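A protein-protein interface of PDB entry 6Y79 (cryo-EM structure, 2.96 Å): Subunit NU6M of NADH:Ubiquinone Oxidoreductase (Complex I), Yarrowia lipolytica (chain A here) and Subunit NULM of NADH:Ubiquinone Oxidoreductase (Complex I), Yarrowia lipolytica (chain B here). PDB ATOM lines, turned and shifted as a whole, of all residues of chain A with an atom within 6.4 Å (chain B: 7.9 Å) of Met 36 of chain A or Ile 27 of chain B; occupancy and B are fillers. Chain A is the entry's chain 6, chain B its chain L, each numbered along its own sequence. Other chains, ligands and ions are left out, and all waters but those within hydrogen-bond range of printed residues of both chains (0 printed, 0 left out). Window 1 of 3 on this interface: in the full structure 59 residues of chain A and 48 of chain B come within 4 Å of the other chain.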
ATOM      1  N   CYS A  19      34.424 -30.085   3.029  1.00  0.00           N
ATOM      2  CA  CYS A  19      33.150 -29.435   3.301  1.00  0.00           C
ATOM      3  C   CYS A  19      32.665 -29.696   4.723  1.00  0.00           C
ATOM      4  O   CYS A  19      32.058 -28.816   5.339  1.00  0.00           O
ATOM      5  CB  CYS A  19      32.112 -29.898   2.287  1.00  0.00           C
ATOM      6  SG  CYS A  19      30.733 -28.785   2.164  1.00  0.00           S
ATOM      7  N   ILE A  23      31.925 -27.082   7.670  1.00  0.00           N
ATOM      8  CA  ILE A  23      30.675 -27.104   8.434  1.00  0.00           C
ATOM      9  C   ILE A  23      30.950 -26.862   9.912  1.00  0.00           C
ATOM     10  O   ILE A  23      30.334 -25.992  10.541  1.00  0.00           O
ATOM     11  CB  ILE A  23      29.924 -28.436   8.226  1.00  0.00           C
ATOM     12  CG1 ILE A  23      29.226 -28.483   6.879  1.00  0.00           C
ATOM     13  CG2 ILE A  23      28.869 -28.649   9.293  1.00  0.00           C
ATOM     14  CD1 ILE A  23      28.852 -29.857   6.459  1.00  0.00           C
ATOM     15  N   PRO A  29      26.196 -19.030  12.173  1.00  0.00           N
ATOM     16  CA  PRO A  29      25.490 -20.318  12.120  1.00  0.00           C
ATOM     17  C   PRO A  29      24.954 -20.703  10.730  1.00  0.00           C
ATOM     18  O   PRO A  29      24.962 -21.888  10.360  1.00  0.00           O
ATOM     19  CB  PRO A  29      24.376 -20.085  13.138  1.00  0.00           C
ATOM     20  CG  PRO A  29      24.385 -18.620  13.484  1.00  0.00           C
ATOM     21  CD  PRO A  29      25.766 -18.216  13.320  1.00  0.00           C
ATOM     22  N   VAL A  31      26.277 -19.663   7.788  1.00  0.00           N
ATOM     23  CA  VAL A  31      27.403 -20.016   6.921  1.00  0.00           C
ATOM     24  C   VAL A  31      27.679 -21.509   7.020  1.00  0.00           C
ATOM     25  O   VAL A  31      27.818 -22.209   6.004  1.00  0.00           O
ATOM     26  CB  VAL A  31      28.615 -19.148   7.305  1.00  0.00           C
ATOM     27  CG1 VAL A  31      29.877 -19.665   6.687  1.00  0.00           C
ATOM     28  CG2 VAL A  31      28.382 -17.690   6.868  1.00  0.00           C
ATOM     29  N   SER A  32      27.631 -22.025   8.249  1.00  0.00           N
ATOM     30  CA  SER A  32      27.674 -23.456   8.513  1.00  0.00           C
ATOM     31  C   SER A  32      26.519 -24.202   7.826  1.00  0.00           C
ATOM     32  O   SER A  32      26.733 -25.264   7.218  1.00  0.00           O
ATOM     33  CB  SER A  32      27.702 -23.637  10.034  1.00  0.00           C
ATOM     34  OG  SER A  32      27.409 -24.916  10.465  1.00  0.00           O
ATOM     35  N   ILE A  33      25.304 -23.649   7.831  1.00  0.00           N
ATOM     36  CA  ILE A  33      24.221 -24.389   7.170  1.00  0.00           C
ATOM     37  C   ILE A  33      24.336 -24.387   5.636  1.00  0.00           C
ATOM     38  O   ILE A  33      23.910 -25.348   4.972  1.00  0.00           O
ATOM     39  CB  ILE A  33      22.858 -23.879   7.643  1.00  0.00           C
ATOM     40  CG1 ILE A  33      21.881 -24.992   7.458  1.00  0.00           C
ATOM     41  CG2 ILE A  33      22.333 -22.746   6.822  1.00  0.00           C
ATOM     42  CD1 ILE A  33      20.831 -24.740   8.210  1.00  0.00           C
ATOM     43  N   LEU A  34      24.940 -23.351   5.043  1.00  0.00           N
ATOM     44  CA  LEU A  34      25.117 -23.357   3.598  1.00  0.00           C
ATOM     45  C   LEU A  34      26.197 -24.337   3.198  1.00  0.00           C
ATOM     46  O   LEU A  34      26.131 -24.941   2.119  1.00  0.00           O
ATOM     47  CB  LEU A  34      25.457 -21.967   3.102  1.00  0.00           C
ATOM     48  CG  LEU A  34      24.355 -20.955   3.326  1.00  0.00           C
ATOM     49  CD1 LEU A  34      24.867 -19.606   2.943  1.00  0.00           C
ATOM     50  CD2 LEU A  34      23.106 -21.344   2.587  1.00  0.00           C
ATOM     51  N   TYR A  35      27.197 -24.513   4.062  1.00  0.00           N
ATOM     52  CA  TYR A  35      28.147 -25.594   3.826  1.00  0.00           C
ATOM     53  C   TYR A  35      27.477 -26.963   3.910  1.00  0.00           C
ATOM     54  O   TYR A  35      27.866 -27.881   3.176  1.00  0.00           O
ATOM     55  CB  TYR A  35      29.311 -25.518   4.804  1.00  0.00           C
ATOM     56  CG  TYR A  35      30.260 -24.380   4.571  1.00  0.00           C
ATOM     57  CD1 TYR A  35      30.844 -24.167   3.333  1.00  0.00           C
ATOM     58  CD2 TYR A  35      30.608 -23.541   5.608  1.00  0.00           C
ATOM     59  CE1 TYR A  35      31.727 -23.121   3.139  1.00  0.00           C
ATOM     60  CE2 TYR A  35      31.488 -22.515   5.428  1.00  0.00           C
ATOM     61  CZ  TYR A  35      32.038 -22.298   4.196  1.00  0.00           C
ATOM     62  OH  TYR A  35      32.913 -21.250   4.046  1.00  0.00           O
ATOM     63  N   MET A  36      26.452 -27.120   4.761  1.00  0.00           N
ATOM     64  CA  MET A  36      25.730 -28.399   4.755  1.00  0.00           C
ATOM     65  C   MET A  36      24.970 -28.622   3.445  1.00  0.00           C
ATOM     66  O   MET A  36      24.948 -29.746   2.923  1.00  0.00           O
ATOM     67  CB  MET A  36      24.764 -28.515   5.930  1.00  0.00           C
ATOM     68  CG  MET A  36      24.226 -29.939   6.051  1.00  0.00           C
ATOM     69  SD  MET A  36      22.750 -30.243   7.031  1.00  0.00           S
ATOM     70  CE  MET A  36      21.730 -28.841   6.607  1.00  0.00           C
ATOM     71  N   ILE A  37      24.350 -27.565   2.903  1.00  0.00           N
ATOM     72  CA  ILE A  37      23.667 -27.672   1.604  1.00  0.00           C
ATOM     73  C   ILE A  37      24.654 -28.046   0.497  1.00  0.00           C
ATOM     74  O   ILE A  37      24.356 -28.873  -0.385  1.00  0.00           O
ATOM     75  CB  ILE A  37      22.930 -26.356   1.286  1.00  0.00           C
ATOM     76  CG1 ILE A  37      21.857 -26.081   2.331  1.00  0.00           C
ATOM     77  CG2 ILE A  37      22.301 -26.383  -0.095  1.00  0.00           C
ATOM     78  CD1 ILE A  37      21.134 -24.781   2.112  1.00  0.00           C
ATOM     79  N   ALA A  38      25.860 -27.479   0.558  1.00  0.00           N
ATOM     80  CA  ALA A  38      26.920 -27.863  -0.369  1.00  0.00           C
ATOM     81  C   ALA A  38      27.310 -29.330  -0.208  1.00  0.00           C
ATOM     82  O   ALA A  38      27.609 -30.007  -1.197  1.00  0.00           O
ATOM     83  CB  ALA A  38      28.133 -26.963  -0.168  1.00  0.00           C
ATOM     84  N   LEU A  39      27.296 -29.840   1.027  1.00  0.00           N
ATOM     85  CA  LEU A  39      27.612 -31.253   1.245  1.00  0.00           C
ATOM     86  C   LEU A  39      26.535 -32.166   0.671  1.00  0.00           C
ATOM     87  O   LEU A  39      26.843 -33.250   0.163  1.00  0.00           O
ATOM     88  CB  LEU A  39      27.806 -31.526   2.735  1.00  0.00           C
ATOM     89  CG  LEU A  39      28.286 -32.927   3.108  1.00  0.00           C
ATOM     90  CD1 LEU A  39      29.600 -33.246   2.432  1.00  0.00           C
ATOM     91  CD2 LEU A  39      28.428 -33.045   4.583  1.00  0.00           C
ATOM     92  N   PHE A  40      25.268 -31.738   0.740  1.00  0.00           N
ATOM     93  CA  PHE A  40      24.189 -32.464   0.063  1.00  0.00           C
ATOM     94  C   PHE A  40      24.416 -32.522  -1.444  1.00  0.00           C
ATOM     95  O   PHE A  40      24.157 -33.550  -2.083  1.00  0.00           O
ATOM     96  CB  PHE A  40      22.837 -31.808   0.333  1.00  0.00           C
ATOM     97  CG  PHE A  40      22.310 -32.013   1.719  1.00  0.00           C
ATOM     98  CD1 PHE A  40      22.012 -33.273   2.181  1.00  0.00           C
ATOM     99  CD2 PHE A  40      22.049 -30.931   2.537  1.00  0.00           C
ATOM    100  CE1 PHE A  40      21.529 -33.466   3.462  1.00  0.00           C
ATOM    101  CE2 PHE A  40      21.552 -31.109   3.807  1.00  0.00           C
ATOM    102  CZ  PHE A  40      21.292 -32.378   4.273  1.00  0.00           C
ATOM    103  N   VAL A  41      24.896 -31.419  -2.027  1.00  0.00           N
ATOM    104  CA  VAL A  41      25.174 -31.393  -3.465  1.00  0.00           C
ATOM    105  C   VAL A  41      26.344 -32.315  -3.821  1.00  0.00           C
ATOM    106  O   VAL A  41      26.309 -33.012  -4.843  1.00  0.00           O
ATOM    107  CB  VAL A  41      25.414 -29.942  -3.921  1.00  0.00           C
ATOM    108  CG1 VAL A  41      25.833 -29.876  -5.370  1.00  0.00           C
ATOM    109  CG2 VAL A  41      24.163 -29.129  -3.723  1.00  0.00           C
ATOM    110  N   TYR A  63      16.087 -33.412   0.768  1.00  0.00           N
ATOM    111  CA  TYR A  63      17.000 -32.899   1.786  1.00  0.00           C
ATOM    112  C   TYR A  63      17.265 -31.414   1.610  1.00  0.00           C
ATOM    113  O   TYR A  63      17.203 -30.648   2.575  1.00  0.00           O
ATOM    114  CB  TYR A  63      18.318 -33.664   1.760  1.00  0.00           C
ATOM    115  CG  TYR A  63      18.235 -35.062   2.304  1.00  0.00           C
ATOM    116  CD1 TYR A  63      17.853 -36.113   1.491  1.00  0.00           C
ATOM    117  CD2 TYR A  63      18.527 -35.331   3.632  1.00  0.00           C
ATOM    118  CE1 TYR A  63      17.769 -37.396   1.980  1.00  0.00           C
ATOM    119  CE2 TYR A  63      18.455 -36.615   4.128  1.00  0.00           C
ATOM    120  CZ  TYR A  63      18.078 -37.642   3.295  1.00  0.00           C
ATOM    121  OH  TYR A  63      18.002 -38.923   3.781  1.00  0.00           O
ATOM    122  N   ILE A  67      14.341 -30.034   4.061  1.00  0.00           N
ATOM    123  CA  ILE A  67      14.992 -30.073   5.366  1.00  0.00           C
ATOM    124  C   ILE A  67      15.880 -28.851   5.558  1.00  0.00           C
ATOM    125  O   ILE A  67      15.861 -28.213   6.620  1.00  0.00           O
ATOM    126  CB  ILE A  67      15.771 -31.391   5.522  1.00  0.00           C
ATOM    127  CG1 ILE A  67      14.807 -32.575   5.539  1.00  0.00           C
ATOM    128  CG2 ILE A  67      16.598 -31.399   6.780  1.00  0.00           C
ATOM    129  CD1 ILE A  67      15.485 -33.909   5.399  1.00  0.00           C
ATOM    130  N   ALA A  68      16.643 -28.481   4.528  1.00  0.00           N
ATOM    131  CA  ALA A  68      17.495 -27.301   4.625  1.00  0.00           C
ATOM    132  C   ALA A  68      16.673 -26.021   4.637  1.00  0.00           C
ATOM    133  O   ALA A  68      17.047 -25.049   5.296  1.00  0.00           O
ATOM    134  CB  ALA A  68      18.499 -27.280   3.480  1.00  0.00           C
ATOM    135  N   PHE A  71      15.413 -25.700   8.099  1.00  0.00           N
ATOM    136  CA  PHE A  71      16.528 -25.343   8.967  1.00  0.00           C
ATOM    137  C   PHE A  71      16.878 -23.852   8.871  1.00  0.00           C
ATOM    138  O   PHE A  71      17.060 -23.174   9.895  1.00  0.00           O
ATOM    139  CB  PHE A  71      17.726 -26.182   8.569  1.00  0.00           C
ATOM    140  CG  PHE A  71      17.764 -27.578   9.102  1.00  0.00           C
ATOM    141  CD1 PHE A  71      16.709 -28.142   9.788  1.00  0.00           C
ATOM    142  CD2 PHE A  71      18.907 -28.336   8.904  1.00  0.00           C
ATOM    143  CE1 PHE A  71      16.793 -29.440  10.237  1.00  0.00           C
ATOM    144  CE2 PHE A  71      18.993 -29.623   9.368  1.00  0.00           C
ATOM    145  CZ  PHE A  71      17.937 -30.171  10.041  1.00  0.00           C
ATOM    146  N   SER B  11      31.327 -36.174  10.812  1.00  0.00           N
ATOM    147  CA  SER B  11      30.056 -35.628  11.268  1.00  0.00           C
ATOM    148  C   SER B  11      29.815 -35.949  12.735  1.00  0.00           C
ATOM    149  O   SER B  11      29.365 -35.092  13.506  1.00  0.00           O
ATOM    150  CB  SER B  11      28.947 -36.201  10.391  1.00  0.00           C
ATOM    151  OG  SER B  11      27.708 -35.589  10.644  1.00  0.00           O
ATOM    152  N   PHE B  15      29.768 -33.339  15.844  1.00  0.00           N
ATOM    153  CA  PHE B  15      28.665 -33.319  16.797  1.00  0.00           C
ATOM    154  C   PHE B  15      29.174 -33.364  18.229  1.00  0.00           C
ATOM    155  O   PHE B  15      28.651 -32.660  19.100  1.00  0.00           O
ATOM    156  CB  PHE B  15      27.731 -34.501  16.536  1.00  0.00           C
ATOM    157  CG  PHE B  15      26.519 -34.536  17.426  1.00  0.00           C
ATOM    158  CD1 PHE B  15      25.368 -33.875  17.062  1.00  0.00           C
ATOM    159  CD2 PHE B  15      26.522 -35.242  18.618  1.00  0.00           C
ATOM    160  CE1 PHE B  15      24.257 -33.913  17.870  1.00  0.00           C
ATOM    161  CE2 PHE B  15      25.427 -35.242  19.428  1.00  0.00           C
ATOM    162  CZ  PHE B  15      24.293 -34.592  19.053  1.00  0.00           C
ATOM    163  N   ASN B  18      31.027 -30.228  19.554  1.00  0.00           N
ATOM    164  CA  ASN B  18      30.272 -28.994  19.413  1.00  0.00           C
ATOM    165  C   ASN B  18      30.100 -28.359  20.781  1.00  0.00           C
ATOM    166  O   ASN B  18      29.472 -28.938  21.670  1.00  0.00           O
ATOM    167  CB  ASN B  18      28.913 -29.279  18.778  1.00  0.00           C
ATOM    168  CG  ASN B  18      28.113 -28.022  18.490  1.00  0.00           C
ATOM    169  OD1 ASN B  18      28.631 -26.911  18.520  1.00  0.00           O
ATOM    170  ND2 ASN B  18      26.830 -28.199  18.215  1.00  0.00           N
ATOM    171  N   ASN B  21      27.240 -23.791  19.306  1.00  0.00           N
ATOM    172  CA  ASN B  21      25.801 -23.525  19.283  1.00  0.00           C
ATOM    173  C   ASN B  21      25.052 -24.849  19.179  1.00  0.00           C
ATOM    174  O   ASN B  21      25.651 -25.926  19.259  1.00  0.00           O
ATOM    175  CB  ASN B  21      25.425 -22.553  18.148  1.00  0.00           C
ATOM    176  CG  ASN B  21      25.975 -22.968  16.803  1.00  0.00           C
ATOM    177  OD1 ASN B  21      26.577 -24.025  16.653  1.00  0.00           O
ATOM    178  ND2 ASN B  21      25.771 -22.121  15.809  1.00  0.00           N
ATOM    179  N   ILE B  22      23.740 -24.763  18.981  1.00  0.00           N
ATOM    180  CA  ILE B  22      22.885 -25.932  18.969  1.00  0.00           C
ATOM    181  C   ILE B  22      22.586 -26.422  17.556  1.00  0.00           C
ATOM    182  O   ILE B  22      22.399 -27.627  17.363  1.00  0.00           O
ATOM    183  CB  ILE B  22      21.579 -25.657  19.755  1.00  0.00           C
ATOM    184  CG1 ILE B  22      20.825 -26.944  20.066  1.00  0.00           C
ATOM    185  CG2 ILE B  22      20.656 -24.692  19.030  1.00  0.00           C
ATOM    186  CD1 ILE B  22      21.613 -27.890  20.887  1.00  0.00           C
ATOM    187  N   ILE B  23      22.591 -25.550  16.551  1.00  0.00           N
ATOM    188  CA  ILE B  23      22.158 -25.992  15.239  1.00  0.00           C
ATOM    189  C   ILE B  23      23.265 -26.709  14.499  1.00  0.00           C
ATOM    190  O   ILE B  23      23.005 -27.406  13.508  1.00  0.00           O
ATOM    191  CB  ILE B  23      21.649 -24.806  14.435  1.00  0.00           C
ATOM    192  CG1 ILE B  23      22.770 -23.820  14.279  1.00  0.00           C
ATOM    193  CG2 ILE B  23      20.502 -24.140  15.156  1.00  0.00           C
ATOM    194  CD1 ILE B  23      22.468 -22.999  13.216  1.00  0.00           C
ATOM    195  N   LEU B  24      24.503 -26.562  14.962  1.00  0.00           N
ATOM    196  CA  LEU B  24      25.566 -27.411  14.462  1.00  0.00           C
ATOM    197  C   LEU B  24      25.309 -28.860  14.842  1.00  0.00           C
ATOM    198  O   LEU B  24      25.614 -29.765  14.069  1.00  0.00           O
ATOM    199  CB  LEU B  24      26.911 -26.926  14.996  1.00  0.00           C
ATOM    200  CG  LEU B  24      28.141 -27.649  14.457  1.00  0.00           C
ATOM    201  CD1 LEU B  24      28.152 -27.600  12.946  1.00  0.00           C
ATOM    202  CD2 LEU B  24      29.415 -27.052  15.030  1.00  0.00           C
ATOM    203  N   ALA B  25      24.683 -29.091  15.993  1.00  0.00           N
ATOM    204  CA  ALA B  25      24.334 -30.442  16.414  1.00  0.00           C
ATOM    205  C   ALA B  25      23.265 -31.050  15.509  1.00  0.00           C
ATOM    206  O   ALA B  25      23.374 -32.221  15.123  1.00  0.00           O
ATOM    207  CB  ALA B  25      23.886 -30.419  17.878  1.00  0.00           C
ATOM    208  N   PHE B  26      22.256 -30.257  15.127  1.00  0.00           N
ATOM    209  CA  PHE B  26      21.236 -30.709  14.179  1.00  0.00           C
ATOM    210  C   PHE B  26      21.836 -31.052  12.827  1.00  0.00           C
ATOM    211  O   PHE B  26      21.522 -32.097  12.237  1.00  0.00           O
ATOM    212  CB  PHE B  26      20.179 -29.634  13.983  1.00  0.00           C
ATOM    213  CG  PHE B  26      19.298 -29.452  15.142  1.00  0.00           C
ATOM    214  CD1 PHE B  26      19.642 -28.562  16.124  1.00  0.00           C
ATOM    215  CD2 PHE B  26      18.124 -30.173  15.264  1.00  0.00           C
ATOM    216  CE1 PHE B  26      18.849 -28.389  17.204  1.00  0.00           C
ATOM    217  CE2 PHE B  26      17.310 -29.990  16.352  1.00  0.00           C
ATOM    218  CZ  PHE B  26      17.672 -29.096  17.326  1.00  0.00           C
ATOM    219  N   ILE B  27      22.690 -30.173  12.306  1.00  0.00           N
ATOM    220  CA  ILE B  27      23.175 -30.438  10.962  1.00  0.00           C
ATOM    221  C   ILE B  27      24.221 -31.546  10.964  1.00  0.00           C
ATOM    222  O   ILE B  27      24.346 -32.277   9.974  1.00  0.00           O
ATOM    223  CB  ILE B  27      23.676 -29.143  10.302  1.00  0.00           C
ATOM    224  CG1 ILE B  27      24.923 -28.618  10.972  1.00  0.00           C
ATOM    225  CG2 ILE B  27      22.576 -28.082  10.297  1.00  0.00           C
ATOM    226  CD1 ILE B  27      25.435 -27.440  10.284  1.00  0.00           C
ATOM    227  N   CYS B  28      24.925 -31.757  12.080  1.00  0.00           N
ATOM    228  CA  CYS B  28      25.819 -32.909  12.159  1.00  0.00           C
ATOM    229  C   CYS B  28      25.040 -34.214  12.249  1.00  0.00           C
ATOM    230  O   CYS B  28      25.467 -35.229  11.685  1.00  0.00           O
ATOM    231  CB  CYS B  28      26.792 -32.763  13.330  1.00  0.00           C
ATOM    232  SG  CYS B  28      28.108 -31.542  13.079  1.00  0.00           S
ATOM    233  N   LEU B  29      23.872 -34.191  12.900  1.00  0.00           N
ATOM    234  CA  LEU B  29      22.972 -35.345  12.890  1.00  0.00           C
ATOM    235  C   LEU B  29      22.504 -35.686  11.474  1.00  0.00           C
ATOM    236  O   LEU B  29      22.514 -36.858  11.057  1.00  0.00           O
ATOM    237  CB  LEU B  29      21.780 -35.050  13.800  1.00  0.00           C
ATOM    238  CG  LEU B  29      20.805 -36.137  14.241  1.00  0.00           C
ATOM    239  CD1 LEU B  29      20.407 -35.912  15.684  1.00  0.00           C
ATOM    240  CD2 LEU B  29      19.570 -36.142  13.357  1.00  0.00           C
ATOM    241  N   GLU B  30      22.104 -34.662  10.714  1.00  0.00           N
ATOM    242  CA  GLU B  30      21.623 -34.900   9.352  1.00  0.00           C
ATOM    243  C   GLU B  30      22.735 -35.393   8.429  1.00  0.00           C
ATOM    244  O   GLU B  30      22.500 -36.249   7.566  1.00  0.00           O
ATOM    245  CB  GLU B  30      20.987 -33.634   8.794  1.00  0.00           C
ATOM    246  CG  GLU B  30      19.761 -33.201   9.557  1.00  0.00           C
ATOM    247  CD  GLU B  30      18.657 -34.242   9.543  1.00  0.00           C
ATOM    248  OE1 GLU B  30      18.394 -34.835   8.476  1.00  0.00           O
ATOM    249  OE2 GLU B  30      18.039 -34.464  10.604  1.00  0.00           O
ATOM    250  N   THR B  31      23.958 -34.893   8.611  1.00  0.00           N
ATOM    251  CA  THR B  31      25.054 -35.378   7.780  1.00  0.00           C
ATOM    252  C   THR B  31      25.484 -36.791   8.163  1.00  0.00           C
ATOM    253  O   THR B  31      25.979 -37.535   7.301  1.00  0.00           O
ATOM    254  CB  THR B  31      26.227 -34.411   7.850  1.00  0.00           C
ATOM    255  OG1 THR B  31      26.567 -34.179   9.216  1.00  0.00           O
ATOM    256  CG2 THR B  31      25.852 -33.097   7.211  1.00  0.00           C
ATOM    257  N   MET B  32      25.296 -37.183   9.431  1.00  0.00           N
ATOM    258  CA  MET B  32      25.458 -38.587   9.815  1.00  0.00           C
ATOM    259  C   MET B  32      24.497 -39.484   9.047  1.00  0.00           C
ATOM    260  O   MET B  32      24.882 -40.554   8.549  1.00  0.00           O
ATOM    261  CB  MET B  32      25.209 -38.773  11.308  1.00  0.00           C
ATOM    262  CG  MET B  32      26.273 -38.323  12.268  1.00  0.00           C
ATOM    263  SD  MET B  32      25.715 -38.816  13.907  1.00  0.00           S
ATOM    264  CE  MET B  32      26.309 -37.487  14.924  1.00  0.00           C
ATOM    265  N   LEU B  33      23.229 -39.069   8.971  1.00  0.00           N
ATOM    266  CA  LEU B  33      22.238 -39.834   8.210  1.00  0.00           C
ATOM    267  C   LEU B  33      22.586 -39.907   6.725  1.00  0.00           C
ATOM    268  O   LEU B  33      22.368 -40.941   6.077  1.00  0.00           O
ATOM    269  CB  LEU B  33      20.859 -39.217   8.395  1.00  0.00           C
ATOM    270  CG  LEU B  33      20.289 -39.449   9.781  1.00  0.00           C
ATOM    271  CD1 LEU B  33      19.247 -38.403  10.100  1.00  0.00           C
ATOM    272  CD2 LEU B  33      19.714 -40.844   9.846  1.00  0.00           C
ATOM    273  N   LEU B  34      23.142 -38.818   6.179  1.00  0.00           N
ATOM    274  CA  LEU B  34      23.647 -38.827   4.806  1.00  0.00           C
ATOM    275  C   LEU B  34      24.746 -39.868   4.609  1.00  0.00           C
ATOM    276  O   LEU B  34      24.762 -40.570   3.593  1.00  0.00           O
ATOM    277  CB  LEU B  34      24.169 -37.441   4.431  1.00  0.00           C
ATOM    278  CG  LEU B  34      24.707 -37.168   3.020  1.00  0.00           C
ATOM    279  CD1 LEU B  34      24.352 -35.792   2.659  1.00  0.00           C
ATOM    280  CD2 LEU B  34      26.210 -37.259   2.917  1.00  0.00           C
ATOM    281  N   LEU B  71      12.799 -30.020  15.308  1.00  0.00           N
ATOM    282  CA  LEU B  71      12.845 -28.572  15.212  1.00  0.00           C
ATOM    283  C   LEU B  71      11.624 -27.942  15.865  1.00  0.00           C
ATOM    284  O   LEU B  71      11.735 -26.851  16.435  1.00  0.00           O
ATOM    285  CB  LEU B  71      13.003 -28.141  13.755  1.00  0.00           C
ATOM    286  CG  LEU B  71      14.455 -27.935  13.288  1.00  0.00           C
ATOM    287  CD1 LEU B  71      15.145 -26.886  14.107  1.00  0.00           C
ATOM    288  CD2 LEU B  71      15.288 -29.178  13.367  1.00  0.00           C
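O of Ile 23 of chain A lies within hydrogen-bond range of OG of Ser 32 of chain A (3.1 Å). O of Asn 21 of chain B is in hydrogen-bond range of ND2 of Asn 18 of chain B, 2.8 Å away. The side-chain sulfur (SG) of Cys 28 of chain B sits at hydrogen-bond distance from the backbone carbonyl oxygen (O) of Leu 24 of chain B (3.2 Å). The side-chain sulfur (SG) of Cys 19 of chain A lies within hydrogen-bond range of the backbone NH (N) of Leu 39 of chain A, at 3.8 Å. The side-chain hydroxyl of Thr 31 of chain B is in hydrogen-bond range of the backbone carbonyl oxygen of Cys 28 of chain B (2.9 Å). The backbone carbonyl oxygen (O) of Ile 27 of chain B is in hydrogen-bond range of the side-chain hydroxyl (OG1) of Thr 31 of chain B (3.0 Å).
Of the 18 printed residues of chain B, 8 touch a printed residue of chain A. Hydrophobic or aromatic side chains of chain B that line the printed part of chain A: Ile 23, Leu 24, Ile 27, Leu 34 and Leu 71. Hydrophobic or aromatic side chains of chain A that line the printed part of chain B: Ile 23, Pro 29, Met 36, Leu 39, Phe 40 and Phe 71.
Among the printed residues, pairs that only touch across the chains: Ile 23 of chain A with Leu 24 of chain B (3.6 Å), Ile 23 of chain A with Ile 27 of chain B (3.8 Å), Pro 29 of chain A with Asn 21 of chain B (3.6 Å), Pro 29 of chain A with Ile 23 of chain B (3.5 Å), Ser 32 of chain A with Leu 24 of chain B (3.7 Å), Ser 32 of chain A with Ile 27 of chain B (3.2 Å), Met 36 of chain A with Ile 27 of chain B (3.6 Å), Met 36 of chain A with Thr 31 of chain B (3.7 Å), Leu 39 of chain A with Thr 31 of chain B (3.7 Å), Phe 40 of chain A with Leu 34 of chain B (3.5 Å), Phe 71 of chain A with Ile 27 of chain B (3.9 Å), Phe 71 of chain A with Glu 30 of chain B (3.6 Å) and Phe 71 of chain A with Leu 71 of chain B (3.5 Å).
Of the printed residues of chain B, Pro 29 of chain A touches Asn 21 and Ile 23. Met 36 of chain A touches just these residues of chain B: Ile 27 (3.6 Å) and Thr 31 (3.7 Å). Printed residues of chain A within 4 Å of Asn 21 of chain B: Pro 29 (3.6 Å). Ile 27 of chain B touches just these residues of chain A: Ile 23 (3.8 Å), Ser 32 (3.2 Å), Met 36 (3.6 Å) and Phe 71 (3.9 Å). Of the printed residues of chain A, Leu 34 of chain B touches Phe 40 (3.5 Å). The nearest residue of chain B that does not touch Met 36 of chain A is Glu 30 of chain B (4.2 Å). The nearest printed residue of chain B that does not touch Leu 39 of chain A is Leu 34 of chain B (4.3 Å).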
